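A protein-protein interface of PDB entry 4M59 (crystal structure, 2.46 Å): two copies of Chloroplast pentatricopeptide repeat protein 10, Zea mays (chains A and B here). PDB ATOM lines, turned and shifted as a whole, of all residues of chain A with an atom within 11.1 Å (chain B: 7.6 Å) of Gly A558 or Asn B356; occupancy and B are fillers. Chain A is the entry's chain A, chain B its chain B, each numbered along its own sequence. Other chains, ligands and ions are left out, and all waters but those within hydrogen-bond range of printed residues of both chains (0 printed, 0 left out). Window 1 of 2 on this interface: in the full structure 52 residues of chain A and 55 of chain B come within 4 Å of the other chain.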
ATOM      1  N   ASN A 525       0.660   3.329  19.704  1.00  0.00           N
ATOM      2  CA  ASN A 525       1.714   3.875  18.890  1.00  0.00           C
ATOM      3  C   ASN A 525       2.673   4.548  19.817  1.00  0.00           C
ATOM      4  O   ASN A 525       2.538   5.730  20.089  1.00  0.00           O
ATOM      5  CB  ASN A 525       1.114   4.911  17.976  1.00  0.00           C
ATOM      6  CG  ASN A 525      -0.171   5.451  18.515  1.00  0.00           C
ATOM      7  OD1 ASN A 525      -1.245   5.125  18.018  1.00  0.00           O
ATOM      8  ND2 ASN A 525      -0.080   6.259  19.564  1.00  0.00           N
ATOM      9  N   PRO A 526       3.650   3.784  20.303  1.00  0.00           N
ATOM     10  CA  PRO A 526       4.591   4.099  21.374  1.00  0.00           C
ATOM     11  C   PRO A 526       5.227   5.464  21.231  1.00  0.00           C
ATOM     12  O   PRO A 526       5.393   5.947  20.124  1.00  0.00           O
ATOM     13  CB  PRO A 526       5.642   3.001  21.239  1.00  0.00           C
ATOM     14  CG  PRO A 526       5.377   2.347  19.952  1.00  0.00           C
ATOM     15  CD  PRO A 526       3.950   2.491  19.693  1.00  0.00           C
ATOM     16  N   ASP A 527       5.637   5.983  22.298  1.00  0.00           N
ATOM     17  CA  ASP A 527       6.224   7.300  22.269  1.00  0.00           C
ATOM     18  C   ASP A 527       7.670   7.231  22.688  1.00  0.00           C
ATOM     19  O   ASP A 527       8.114   6.225  23.200  1.00  0.00           O
ATOM     20  CB  ASP A 527       5.436   8.239  23.169  1.00  0.00           C
ATOM     21  CG  ASP A 527       6.042   8.391  24.526  1.00  0.00           C
ATOM     22  OD1 ASP A 527       6.949   9.227  24.665  1.00  0.00           O
ATOM     23  OD2 ASP A 527       5.601   7.701  25.462  1.00  0.00           O
ATOM     24  N   LEU A 528       8.403   8.315  22.481  1.00  0.00           N
ATOM     25  CA  LEU A 528       9.846   8.313  22.656  1.00  0.00           C
ATOM     26  C   LEU A 528      10.280   7.928  24.056  1.00  0.00           C
ATOM     27  O   LEU A 528      11.340   7.344  24.257  1.00  0.00           O
ATOM     28  CB  LEU A 528      10.414   9.679  22.315  1.00  0.00           C
ATOM     29  CG  LEU A 528      11.926   9.718  22.143  1.00  0.00           C
ATOM     30  CD1 LEU A 528      12.301   8.907  20.947  1.00  0.00           C
ATOM     31  CD2 LEU A 528      12.384  11.126  21.980  1.00  0.00           C
ATOM     32  N   PHE A 531      10.116   4.092  23.951  1.00  0.00           N
ATOM     33  CA  PHE A 531      11.178   3.545  23.142  1.00  0.00           C
ATOM     34  C   PHE A 531      12.498   3.616  23.873  1.00  0.00           C
ATOM     35  O   PHE A 531      13.141   2.607  24.093  1.00  0.00           O
ATOM     36  CB  PHE A 531      11.299   4.333  21.847  1.00  0.00           C
ATOM     37  CG  PHE A 531      10.210   4.062  20.848  1.00  0.00           C
ATOM     38  CD1 PHE A 531      10.178   2.886  20.138  1.00  0.00           C
ATOM     39  CD2 PHE A 531       9.248   5.007  20.585  1.00  0.00           C
ATOM     40  CE1 PHE A 531       9.197   2.649  19.212  1.00  0.00           C
ATOM     41  CE2 PHE A 531       8.270   4.765  19.660  1.00  0.00           C
ATOM     42  CZ  PHE A 531       8.253   3.596  18.971  1.00  0.00           C
ATOM     43  N   GLU A 549      17.234  -3.153  17.648  1.00  0.00           N
ATOM     44  CA  GLU A 549      15.967  -3.333  16.985  1.00  0.00           C
ATOM     45  C   GLU A 549      15.014  -2.257  17.432  1.00  0.00           C
ATOM     46  O   GLU A 549      14.171  -1.821  16.669  1.00  0.00           O
ATOM     47  CB  GLU A 549      15.386  -4.710  17.292  1.00  0.00           C
ATOM     48  CG  GLU A 549      14.935  -5.470  16.063  1.00  0.00           C
ATOM     49  CD  GLU A 549      14.358  -6.823  16.413  1.00  0.00           C
ATOM     50  OE1 GLU A 549      14.261  -7.132  17.616  1.00  0.00           O
ATOM     51  OE2 GLU A 549      13.998  -7.577  15.490  1.00  0.00           O
ATOM     52  N   VAL A 550      15.183  -1.821  18.665  1.00  0.00           N
ATOM     53  CA  VAL A 550      14.358  -0.759  19.195  1.00  0.00           C
ATOM     54  C   VAL A 550      14.708   0.567  18.555  1.00  0.00           C
ATOM     55  O   VAL A 550      13.850   1.322  18.176  1.00  0.00           O
ATOM     56  CB  VAL A 550      14.512  -0.652  20.703  1.00  0.00           C
ATOM     57  CG1 VAL A 550      13.756   0.508  21.238  1.00  0.00           C
ATOM     58  CG2 VAL A 550      14.015  -1.879  21.338  1.00  0.00           C
ATOM     59  N   PHE A 551      15.991   0.822  18.427  1.00  0.00           N
ATOM     60  CA  PHE A 551      16.492   2.046  17.834  1.00  0.00           C
ATOM     61  C   PHE A 551      15.974   2.248  16.420  1.00  0.00           C
ATOM     62  O   PHE A 551      15.524   3.326  16.061  1.00  0.00           O
ATOM     63  CB  PHE A 551      18.011   2.020  17.820  1.00  0.00           C
ATOM     64  CG  PHE A 551      18.639   3.251  17.258  1.00  0.00           C
ATOM     65  CD1 PHE A 551      18.817   4.364  18.031  1.00  0.00           C
ATOM     66  CD2 PHE A 551      19.077   3.282  15.961  1.00  0.00           C
ATOM     67  CE1 PHE A 551      19.397   5.478  17.519  1.00  0.00           C
ATOM     68  CE2 PHE A 551      19.660   4.400  15.450  1.00  0.00           C
ATOM     69  CZ  PHE A 551      19.817   5.495  16.228  1.00  0.00           C
ATOM     70  N   ASP A 552      16.048   1.206  15.613  1.00  0.00           N
ATOM     71  CA  ASP A 552      15.585   1.313  14.250  1.00  0.00           C
ATOM     72  C   ASP A 552      14.089   1.454  14.265  1.00  0.00           C
ATOM     73  O   ASP A 552      13.521   2.220  13.506  1.00  0.00           O
ATOM     74  CB  ASP A 552      15.988   0.077  13.462  1.00  0.00           C
ATOM     75  CG  ASP A 552      17.482  -0.136  13.451  1.00  0.00           C
ATOM     76  OD1 ASP A 552      18.217   0.785  13.847  1.00  0.00           O
ATOM     77  OD2 ASP A 552      17.925  -1.226  13.025  1.00  0.00           O
ATOM     78  N   SER A 553      13.454   0.725  15.159  1.00  0.00           N
ATOM     79  CA  SER A 553      12.020   0.780  15.262  1.00  0.00           C
ATOM     80  C   SER A 553      11.567   2.131  15.738  1.00  0.00           C
ATOM     81  O   SER A 553      10.399   2.457  15.639  1.00  0.00           O
ATOM     82  CB  SER A 553      11.508  -0.290  16.200  1.00  0.00           C
ATOM     83  OG  SER A 553      11.200  -1.469  15.485  1.00  0.00           O
ATOM     84  N   ILE A 554      12.487   2.911  16.284  1.00  0.00           N
ATOM     85  CA  ILE A 554      12.192   4.292  16.594  1.00  0.00           C
ATOM     86  C   ILE A 554      12.186   5.000  15.267  1.00  0.00           C
ATOM     87  O   ILE A 554      11.307   5.804  14.978  1.00  0.00           O
ATOM     88  CB  ILE A 554      13.282   4.923  17.469  1.00  0.00           C
ATOM     89  CG1 ILE A 554      13.196   4.409  18.900  1.00  0.00           C
ATOM     90  CG2 ILE A 554      13.177   6.434  17.484  1.00  0.00           C
ATOM     91  CD1 ILE A 554      14.267   4.948  19.786  1.00  0.00           C
ATOM     92  N   LYS A 555      13.186   4.700  14.447  1.00  0.00           N
ATOM     93  CA  LYS A 555      13.304   5.312  13.127  1.00  0.00           C
ATOM     94  C   LYS A 555      12.122   4.936  12.240  1.00  0.00           C
ATOM     95  O   LYS A 555      11.545   5.792  11.565  1.00  0.00           O
ATOM     96  CB  LYS A 555      14.616   4.895  12.461  1.00  0.00           C
ATOM     97  CG  LYS A 555      15.843   5.609  13.004  1.00  0.00           C
ATOM     98  CD  LYS A 555      17.075   5.296  12.173  1.00  0.00           C
ATOM     99  CE  LYS A 555      17.720   3.990  12.607  1.00  0.00           C
ATOM    100  NZ  LYS A 555      19.035   3.771  11.945  1.00  0.00           N
ATOM    101  N   ARG A 556      11.764   3.657  12.249  1.00  0.00           N
ATOM    102  CA  ARG A 556      10.648   3.170  11.446  1.00  0.00           C
ATOM    103  C   ARG A 556       9.323   3.743  11.938  1.00  0.00           C
ATOM    104  O   ARG A 556       8.309   3.667  11.247  1.00  0.00           O
ATOM    105  CB  ARG A 556      10.603   1.640  11.471  1.00  0.00           C
ATOM    106  CG  ARG A 556      11.916   0.970  11.107  1.00  0.00           C
ATOM    107  CD  ARG A 556      11.775   0.119   9.854  1.00  0.00           C
ATOM    108  NE  ARG A 556      13.013   0.075   9.081  1.00  0.00           N
ATOM    109  CZ  ARG A 556      13.398  -0.967   8.351  1.00  0.00           C
ATOM    110  NH1 ARG A 556      12.648  -2.058   8.296  1.00  0.00           N
ATOM    111  NH2 ARG A 556      14.540  -0.922   7.678  1.00  0.00           N
ATOM    112  N   SER A 557       9.342   4.316  13.135  1.00  0.00           N
ATOM    113  CA  SER A 557       8.146   4.904  13.724  1.00  0.00           C
ATOM    114  C   SER A 557       7.913   6.318  13.201  1.00  0.00           C
ATOM    115  O   SER A 557       6.792   6.689  12.859  1.00  0.00           O
ATOM    116  CB  SER A 557       8.245   4.916  15.248  1.00  0.00           C
ATOM    117  OG  SER A 557       7.075   5.460  15.830  1.00  0.00           O
ATOM    118  N   GLY A 558       8.983   7.107  13.144  1.00  0.00           N
ATOM    119  CA  GLY A 558       8.901   8.476  12.669  1.00  0.00           C
ATOM    120  C   GLY A 558       9.062   9.488  13.785  1.00  0.00           C
ATOM    121  O   GLY A 558       8.356  10.498  13.825  1.00  0.00           O
ATOM    122  N   LEU A 559       9.991   9.220  14.694  1.00  0.00           N
ATOM    123  CA  LEU A 559      10.243  10.113  15.808  1.00  0.00           C
ATOM    124  C   LEU A 559      11.689  10.556  15.760  1.00  0.00           C
ATOM    125  O   LEU A 559      12.499   9.967  15.063  1.00  0.00           O
ATOM    126  CB  LEU A 559       9.897   9.452  17.145  1.00  0.00           C
ATOM    127  CG  LEU A 559       8.439   9.625  17.574  1.00  0.00           C
ATOM    128  CD1 LEU A 559       7.550   8.697  16.801  1.00  0.00           C
ATOM    129  CD2 LEU A 559       8.248   9.409  19.050  1.00  0.00           C
ATOM    130  N   SER A 560      11.998  11.618  16.481  1.00  0.00           N
ATOM    131  CA  SER A 560      13.342  12.157  16.461  1.00  0.00           C
ATOM    132  C   SER A 560      14.100  11.759  17.715  1.00  0.00           C
ATOM    133  O   SER A 560      13.743  12.170  18.804  1.00  0.00           O
ATOM    134  CB  SER A 560      13.295  13.680  16.342  1.00  0.00           C
ATOM    135  OG  SER A 560      13.921  14.126  15.150  1.00  0.00           O
ATOM    136  N   PRO A 561      15.147  10.955  17.553  1.00  0.00           N
ATOM    137  CA  PRO A 561      16.010  10.504  18.630  1.00  0.00           C
ATOM    138  C   PRO A 561      16.669  11.668  19.326  1.00  0.00           C
ATOM    139  O   PRO A 561      17.427  12.387  18.696  1.00  0.00           O
ATOM    140  CB  PRO A 561      17.082   9.722  17.890  1.00  0.00           C
ATOM    141  CG  PRO A 561      16.466   9.300  16.667  1.00  0.00           C
ATOM    142  CD  PRO A 561      15.563  10.392  16.268  1.00  0.00           C
ATOM    143  N   ASP A 562      16.404  11.857  20.609  1.00  0.00           N
ATOM    144  CA  ASP A 562      17.080  12.906  21.340  1.00  0.00           C
ATOM    145  C   ASP A 562      18.383  12.393  21.904  1.00  0.00           C
ATOM    146  O   ASP A 562      18.810  11.305  21.580  1.00  0.00           O
ATOM    147  CB  ASP A 562      16.195  13.469  22.437  1.00  0.00           C
ATOM    148  CG  ASP A 562      15.664  12.419  23.350  1.00  0.00           C
ATOM    149  OD1 ASP A 562      16.214  11.310  23.368  1.00  0.00           O
ATOM    150  OD2 ASP A 562      14.686  12.700  24.067  1.00  0.00           O
ATOM    151  N   ASN B 321      15.245  18.980   8.305  1.00  0.00           N
ATOM    152  CA  ASN B 321      14.144  18.357   9.025  1.00  0.00           C
ATOM    153  C   ASN B 321      13.647  19.259  10.144  1.00  0.00           C
ATOM    154  O   ASN B 321      12.479  19.210  10.522  1.00  0.00           O
ATOM    155  CB  ASN B 321      14.571  17.004   9.591  1.00  0.00           C
ATOM    156  CG  ASN B 321      14.675  15.934   8.524  1.00  0.00           C
ATOM    157  OD1 ASN B 321      14.194  16.109   7.405  1.00  0.00           O
ATOM    158  ND2 ASN B 321      15.306  14.819   8.866  1.00  0.00           N
ATOM    159  N   ASN B 351      15.584  11.711   4.566  1.00  0.00           N
ATOM    160  CA  ASN B 351      15.517  10.453   5.281  1.00  0.00           C
ATOM    161  C   ASN B 351      14.092  10.105   5.650  1.00  0.00           C
ATOM    162  O   ASN B 351      13.175  10.748   5.193  1.00  0.00           O
ATOM    163  CB  ASN B 351      16.438  10.472   6.502  1.00  0.00           C
ATOM    164  CG  ASN B 351      16.016  11.457   7.555  1.00  0.00           C
ATOM    165  OD1 ASN B 351      15.349  12.439   7.273  1.00  0.00           O
ATOM    166  ND2 ASN B 351      16.417  11.200   8.782  1.00  0.00           N
ATOM    167  N   ARG B 352      13.875   9.123   6.490  1.00  0.00           N
ATOM    168  CA  ARG B 352      12.523   8.807   6.863  1.00  0.00           C
ATOM    169  C   ARG B 352      11.925   9.908   7.657  1.00  0.00           C
ATOM    170  O   ARG B 352      10.748  10.168   7.609  1.00  0.00           O
ATOM    171  CB  ARG B 352      12.475   7.588   7.744  1.00  0.00           C
ATOM    172  CG  ARG B 352      12.967   6.405   7.103  1.00  0.00           C
ATOM    173  CD  ARG B 352      12.584   5.185   7.890  1.00  0.00           C
ATOM    174  NE  ARG B 352      13.685   4.682   8.701  1.00  0.00           N
ATOM    175  CZ  ARG B 352      14.879   4.340   8.233  1.00  0.00           C
ATOM    176  NH1 ARG B 352      15.796   3.899   9.059  1.00  0.00           N
ATOM    177  NH2 ARG B 352      15.158   4.418   6.935  1.00  0.00           N
ATOM    178  N   VAL B 353      12.752  10.535   8.434  1.00  0.00           N
ATOM    179  CA  VAL B 353      12.283  11.564   9.335  1.00  0.00           C
ATOM    180  C   VAL B 353      11.745  12.721   8.538  1.00  0.00           C
ATOM    181  O   VAL B 353      10.868  13.441   8.976  1.00  0.00           O
ATOM    182  CB  VAL B 353      13.425  12.044  10.213  1.00  0.00           C
ATOM    183  CG1 VAL B 353      12.921  12.991  11.254  1.00  0.00           C
ATOM    184  CG2 VAL B 353      14.074  10.882  10.881  1.00  0.00           C
ATOM    185  N   THR B 354      12.280  12.893   7.345  1.00  0.00           N
ATOM    186  CA  THR B 354      11.913  14.002   6.500  1.00  0.00           C
ATOM    187  C   THR B 354      10.492  13.881   6.024  1.00  0.00           C
ATOM    188  O   THR B 354       9.692  14.776   6.217  1.00  0.00           O
ATOM    189  CB  THR B 354      12.827  14.082   5.304  1.00  0.00           C
ATOM    190  OG1 THR B 354      14.143  14.394   5.758  1.00  0.00           O
ATOM    191  CG2 THR B 354      12.389  15.165   4.391  1.00  0.00           C
ATOM    192  N   TRP B 355      10.180  12.757   5.401  1.00  0.00           N
ATOM    193  CA  TRP B 355       8.856  12.540   4.874  1.00  0.00           C
ATOM    194  C   TRP B 355       7.841  12.568   5.986  1.00  0.00           C
ATOM    195  O   TRP B 355       6.741  13.054   5.810  1.00  0.00           O
ATOM    196  CB  TRP B 355       8.790  11.215   4.133  1.00  0.00           C
ATOM    197  CG  TRP B 355       9.755  11.109   3.031  1.00  0.00           C
ATOM    198  CD1 TRP B 355      10.830  10.301   2.978  1.00  0.00           C
ATOM    199  CD2 TRP B 355       9.745  11.847   1.814  1.00  0.00           C
ATOM    200  NE1 TRP B 355      11.500  10.476   1.803  1.00  0.00           N
ATOM    201  CE2 TRP B 355      10.852  11.427   1.067  1.00  0.00           C
ATOM    202  CE3 TRP B 355       8.909  12.822   1.284  1.00  0.00           C
ATOM    203  CZ2 TRP B 355      11.137  11.940  -0.178  1.00  0.00           C
ATOM    204  CZ3 TRP B 355       9.201  13.329   0.054  1.00  0.00           C
ATOM    205  CH2 TRP B 355      10.302  12.893  -0.667  1.00  0.00           C
ATOM    206  N   ASN B 356       8.214  12.049   7.140  1.00  0.00           N
ATOM    207  CA  ASN B 356       7.317  12.020   8.269  1.00  0.00           C
ATOM    208  C   ASN B 356       7.062  13.422   8.723  1.00  0.00           C
ATOM    209  O   ASN B 356       6.017  13.746   9.247  1.00  0.00           O
ATOM    210  CB  ASN B 356       7.950  11.242   9.408  1.00  0.00           C
ATOM    211  CG  ASN B 356       7.175  10.006   9.766  1.00  0.00           C
ATOM    212  OD1 ASN B 356       7.371   8.951   9.180  1.00  0.00           O
ATOM    213  ND2 ASN B 356       6.295  10.128  10.743  1.00  0.00           N
ATOM    214  N   THR B 357       8.060  14.256   8.518  1.00  0.00           N
ATOM    215  CA  THR B 357       7.988  15.647   8.894  1.00  0.00           C
ATOM    216  C   THR B 357       7.113  16.378   7.908  1.00  0.00           C
ATOM    217  O   THR B 357       6.288  17.202   8.283  1.00  0.00           O
ATOM    218  CB  THR B 357       9.379  16.280   8.896  1.00  0.00           C
ATOM    219  OG1 THR B 357      10.157  15.722   9.958  1.00  0.00           O
ATOM    220  CG2 THR B 357       9.281  17.752   9.080  1.00  0.00           C
ATOM    221  N   MET B 358       7.279  16.053   6.637  1.00  0.00           N
ATOM    222  CA  MET B 358       6.506  16.707   5.611  1.00  0.00           C
ATOM    223  C   MET B 358       5.079  16.246   5.612  1.00  0.00           C
ATOM    224  O   MET B 358       4.248  16.821   4.934  1.00  0.00           O
ATOM    225  CB  MET B 358       7.143  16.507   4.249  1.00  0.00           C
ATOM    226  CG  MET B 358       8.529  17.052   4.180  1.00  0.00           C
ATOM    227  SD  MET B 358       9.002  17.522   2.548  1.00  0.00           S
ATOM    228  CE  MET B 358       7.736  18.713   2.264  1.00  0.00           C
ATOM    229  N   LEU B 359       4.786  15.225   6.397  1.00  0.00           N
ATOM    230  CA  LEU B 359       3.448  14.666   6.438  1.00  0.00           C
ATOM    231  C   LEU B 359       2.742  14.896   7.766  1.00  0.00           C
ATOM    232  O   LEU B 359       1.581  14.557   7.927  1.00  0.00           O
ATOM    233  CB  LEU B 359       3.495  13.179   6.117  1.00  0.00           C
ATOM    234  CG  LEU B 359       3.801  12.817   4.672  1.00  0.00           C
ATOM    235  CD1 LEU B 359       4.083  11.359   4.527  1.00  0.00           C
ATOM    236  CD2 LEU B 359       2.632  13.193   3.826  1.00  0.00           C
ATOM    237  N   ALA B 360       3.451  15.478   8.719  1.00  0.00           N
ATOM    238  CA  ALA B 360       2.883  15.728  10.023  1.00  0.00           C
ATOM    239  C   ALA B 360       2.426  17.156  10.108  1.00  0.00           C
ATOM    240  O   ALA B 360       2.516  17.786  11.146  1.00  0.00           O
ATOM    241  CB  ALA B 360       3.887  15.455  11.079  1.00  0.00           C
ATOM    242  N   VAL B 361       1.935  17.671   8.998  1.00  0.00           N
ATOM    243  CA  VAL B 361       1.508  19.041   8.955  1.00  0.00           C
ATOM    244  C   VAL B 361       0.198  19.224   9.670  1.00  0.00           C
ATOM    245  O   VAL B 361      -0.733  18.466   9.480  1.00  0.00           O
ATOM    246  CB  VAL B 361       1.339  19.525   7.527  1.00  0.00           C
ATOM    247  CG1 VAL B 361       2.642  20.015   6.989  1.00  0.00           C
ATOM    248  CG2 VAL B 361       0.812  18.423   6.675  1.00  0.00           C
ATOM    249  N   VAL B 374       3.955  15.435  -2.001  1.00  0.00           N
ATOM    250  CA  VAL B 374       4.990  14.831  -1.184  1.00  0.00           C
ATOM    251  C   VAL B 374       5.141  13.385  -1.577  1.00  0.00           C
ATOM    252  O   VAL B 374       6.238  12.888  -1.738  1.00  0.00           O
ATOM    253  CB  VAL B 374       4.642  14.907   0.282  1.00  0.00           C
ATOM    254  CG1 VAL B 374       5.725  14.277   1.094  1.00  0.00           C
ATOM    255  CG2 VAL B 374       4.462  16.327   0.697  1.00  0.00           C
ATOM    256  N   MET B 378       8.082  11.174  -3.045  1.00  0.00           N
ATOM    257  CA  MET B 378       8.380  10.092  -2.130  1.00  0.00           C
ATOM    258  C   MET B 378       8.427   8.796  -2.919  1.00  0.00           C
ATOM    259  O   MET B 378       8.987   7.801  -2.463  1.00  0.00           O
ATOM    260  CB  MET B 378       7.297  10.003  -1.056  1.00  0.00           C
ATOM    261  CG  MET B 378       7.780   9.484   0.285  1.00  0.00           C
ATOM    262  SD  MET B 378       6.420   9.216   1.434  1.00  0.00           S
ATOM    263  CE  MET B 378       5.447  10.693   1.163  1.00  0.00           C
ATOM    264  N   SER B 386       6.881   1.650   3.476  1.00  0.00           N
ATOM    265  CA  SER B 386       6.735   0.624   4.489  1.00  0.00           C
ATOM    266  C   SER B 386       5.287   0.534   4.859  1.00  0.00           C
ATOM    267  O   SER B 386       4.455   1.141   4.232  1.00  0.00           O
ATOM    268  CB  SER B 386       7.522   0.998   5.729  1.00  0.00           C
ATOM    269  OG  SER B 386       6.867   2.023   6.440  1.00  0.00           O
ATOM    270  N   ASP B 388       4.234   1.413   7.904  1.00  0.00           N
ATOM    271  CA  ASP B 388       3.966   2.548   8.749  1.00  0.00           C
ATOM    272  C   ASP B 388       3.936   3.800   7.907  1.00  0.00           C
ATOM    273  O   ASP B 388       3.287   4.773   8.253  1.00  0.00           O
ATOM    274  CB  ASP B 388       5.000   2.636   9.841  1.00  0.00           C
ATOM    275  N   THR B 389       4.639   3.760   6.787  1.00  0.00           N
ATOM    276  CA  THR B 389       4.632   4.854   5.837  1.00  0.00           C
ATOM    277  C   THR B 389       3.250   5.067   5.260  1.00  0.00           C
ATOM    278  O   THR B 389       2.790   6.194   5.157  1.00  0.00           O
ATOM    279  CB  THR B 389       5.562   4.575   4.683  1.00  0.00           C
ATOM    280  OG1 THR B 389       6.874   4.330   5.184  1.00  0.00           O
ATOM    281  CG2 THR B 389       5.605   5.747   3.759  1.00  0.00           C
ATOM    282  N   THR B 392       0.920   6.535   7.662  1.00  0.00           N
ATOM    283  CA  THR B 392       1.199   7.934   7.833  1.00  0.00           C
ATOM    284  C   THR B 392       0.556   8.690   6.690  1.00  0.00           C
ATOM    285  O   THR B 392       0.043   9.784   6.872  1.00  0.00           O
ATOM    286  CB  THR B 392       2.693   8.169   7.862  1.00  0.00           C
ATOM    287  OG1 THR B 392       3.271   7.291   8.823  1.00  0.00           O
ATOM    288  CG2 THR B 392       2.993   9.570   8.270  1.00  0.00           C
ATOM    289  N   ARG B 399      -6.569  13.968   7.712  1.00  0.00           N
ATOM    290  CA  ARG B 399      -6.598  15.297   8.291  1.00  0.00           C
ATOM    291  C   ARG B 399      -7.307  16.237   7.332  1.00  0.00           C
ATOM    292  O   ARG B 399      -8.229  16.947   7.716  1.00  0.00           O
ATOM    293  CB  ARG B 399      -5.180  15.795   8.559  1.00  0.00           C
ATOM    294  CG  ARG B 399      -4.678  15.538   9.969  1.00  0.00           C
ATOM    295  CD  ARG B 399      -3.179  15.771  10.067  1.00  0.00           C
ATOM    296  NE  ARG B 399      -2.438  14.515  10.036  1.00  0.00           N
ATOM    297  CZ  ARG B 399      -1.202  14.388   9.570  1.00  0.00           C
ATOM    298  NH1 ARG B 399      -0.560  15.443   9.095  1.00  0.00           N
ATOM    299  NH2 ARG B 399      -0.608  13.204   9.581  1.00  0.00           N
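Of the 19 printed residues of chain B, 3 touch a printed residue of chain A. Printed residues of chain B that touch a printed residue of chain A: Arg B352, Asn B356 and Asp B388. Of the 19 printed residues of chain A, 3 touch a printed residue of chain B.
The side-chain carboxylate of Asp A552 lies within salt-bridge range of the side-chain amino group of Lys A555, at 3.6 Å. OG of Ser B386 lies within hydrogen-bond range of N of Asp B388, 3.1 Å away. O of Asp B388 lies within hydrogen-bond range of OG1 of Thr B392, at 2.6 Å.
Arg B352 touches Lys A555. Arg A556 touches Asp B388. Gly A558 touches Asn B356 (CA to ND2, 3.6 Å).
No position is printed for both chains. Of the 3 pairs that touch across the chains among the printed residues, none has its exchanged pair printed and touching as well.
No residue of chain A comes within 4 Å of Val B353. Thr B354 touches none of the printed residues of chain A. No residue of chain A comes within 4 Å of Thr B357. No residue of chain A comes within 4 Å of Leu B359. Ala B360 touches none of the printed residues of chain A. No residue of chain A comes within 4 Å of Thr B389. Of the printed residues of chain B, Lys A555 touches Arg B352 (3.6 Å). Of the printed residues of chain A, Arg B352 touches Lys A555 (3.6 Å). Of the printed residues of chain B, Arg A556 touches Asp B388 (3.7 Å). The nearest printed residue of chain B that does not touch Gly A558 is Arg B352 (5.6 Å). The nearest printed residue of chain A that does not touch Asp B388 is Ser A557 (5.4 Å).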
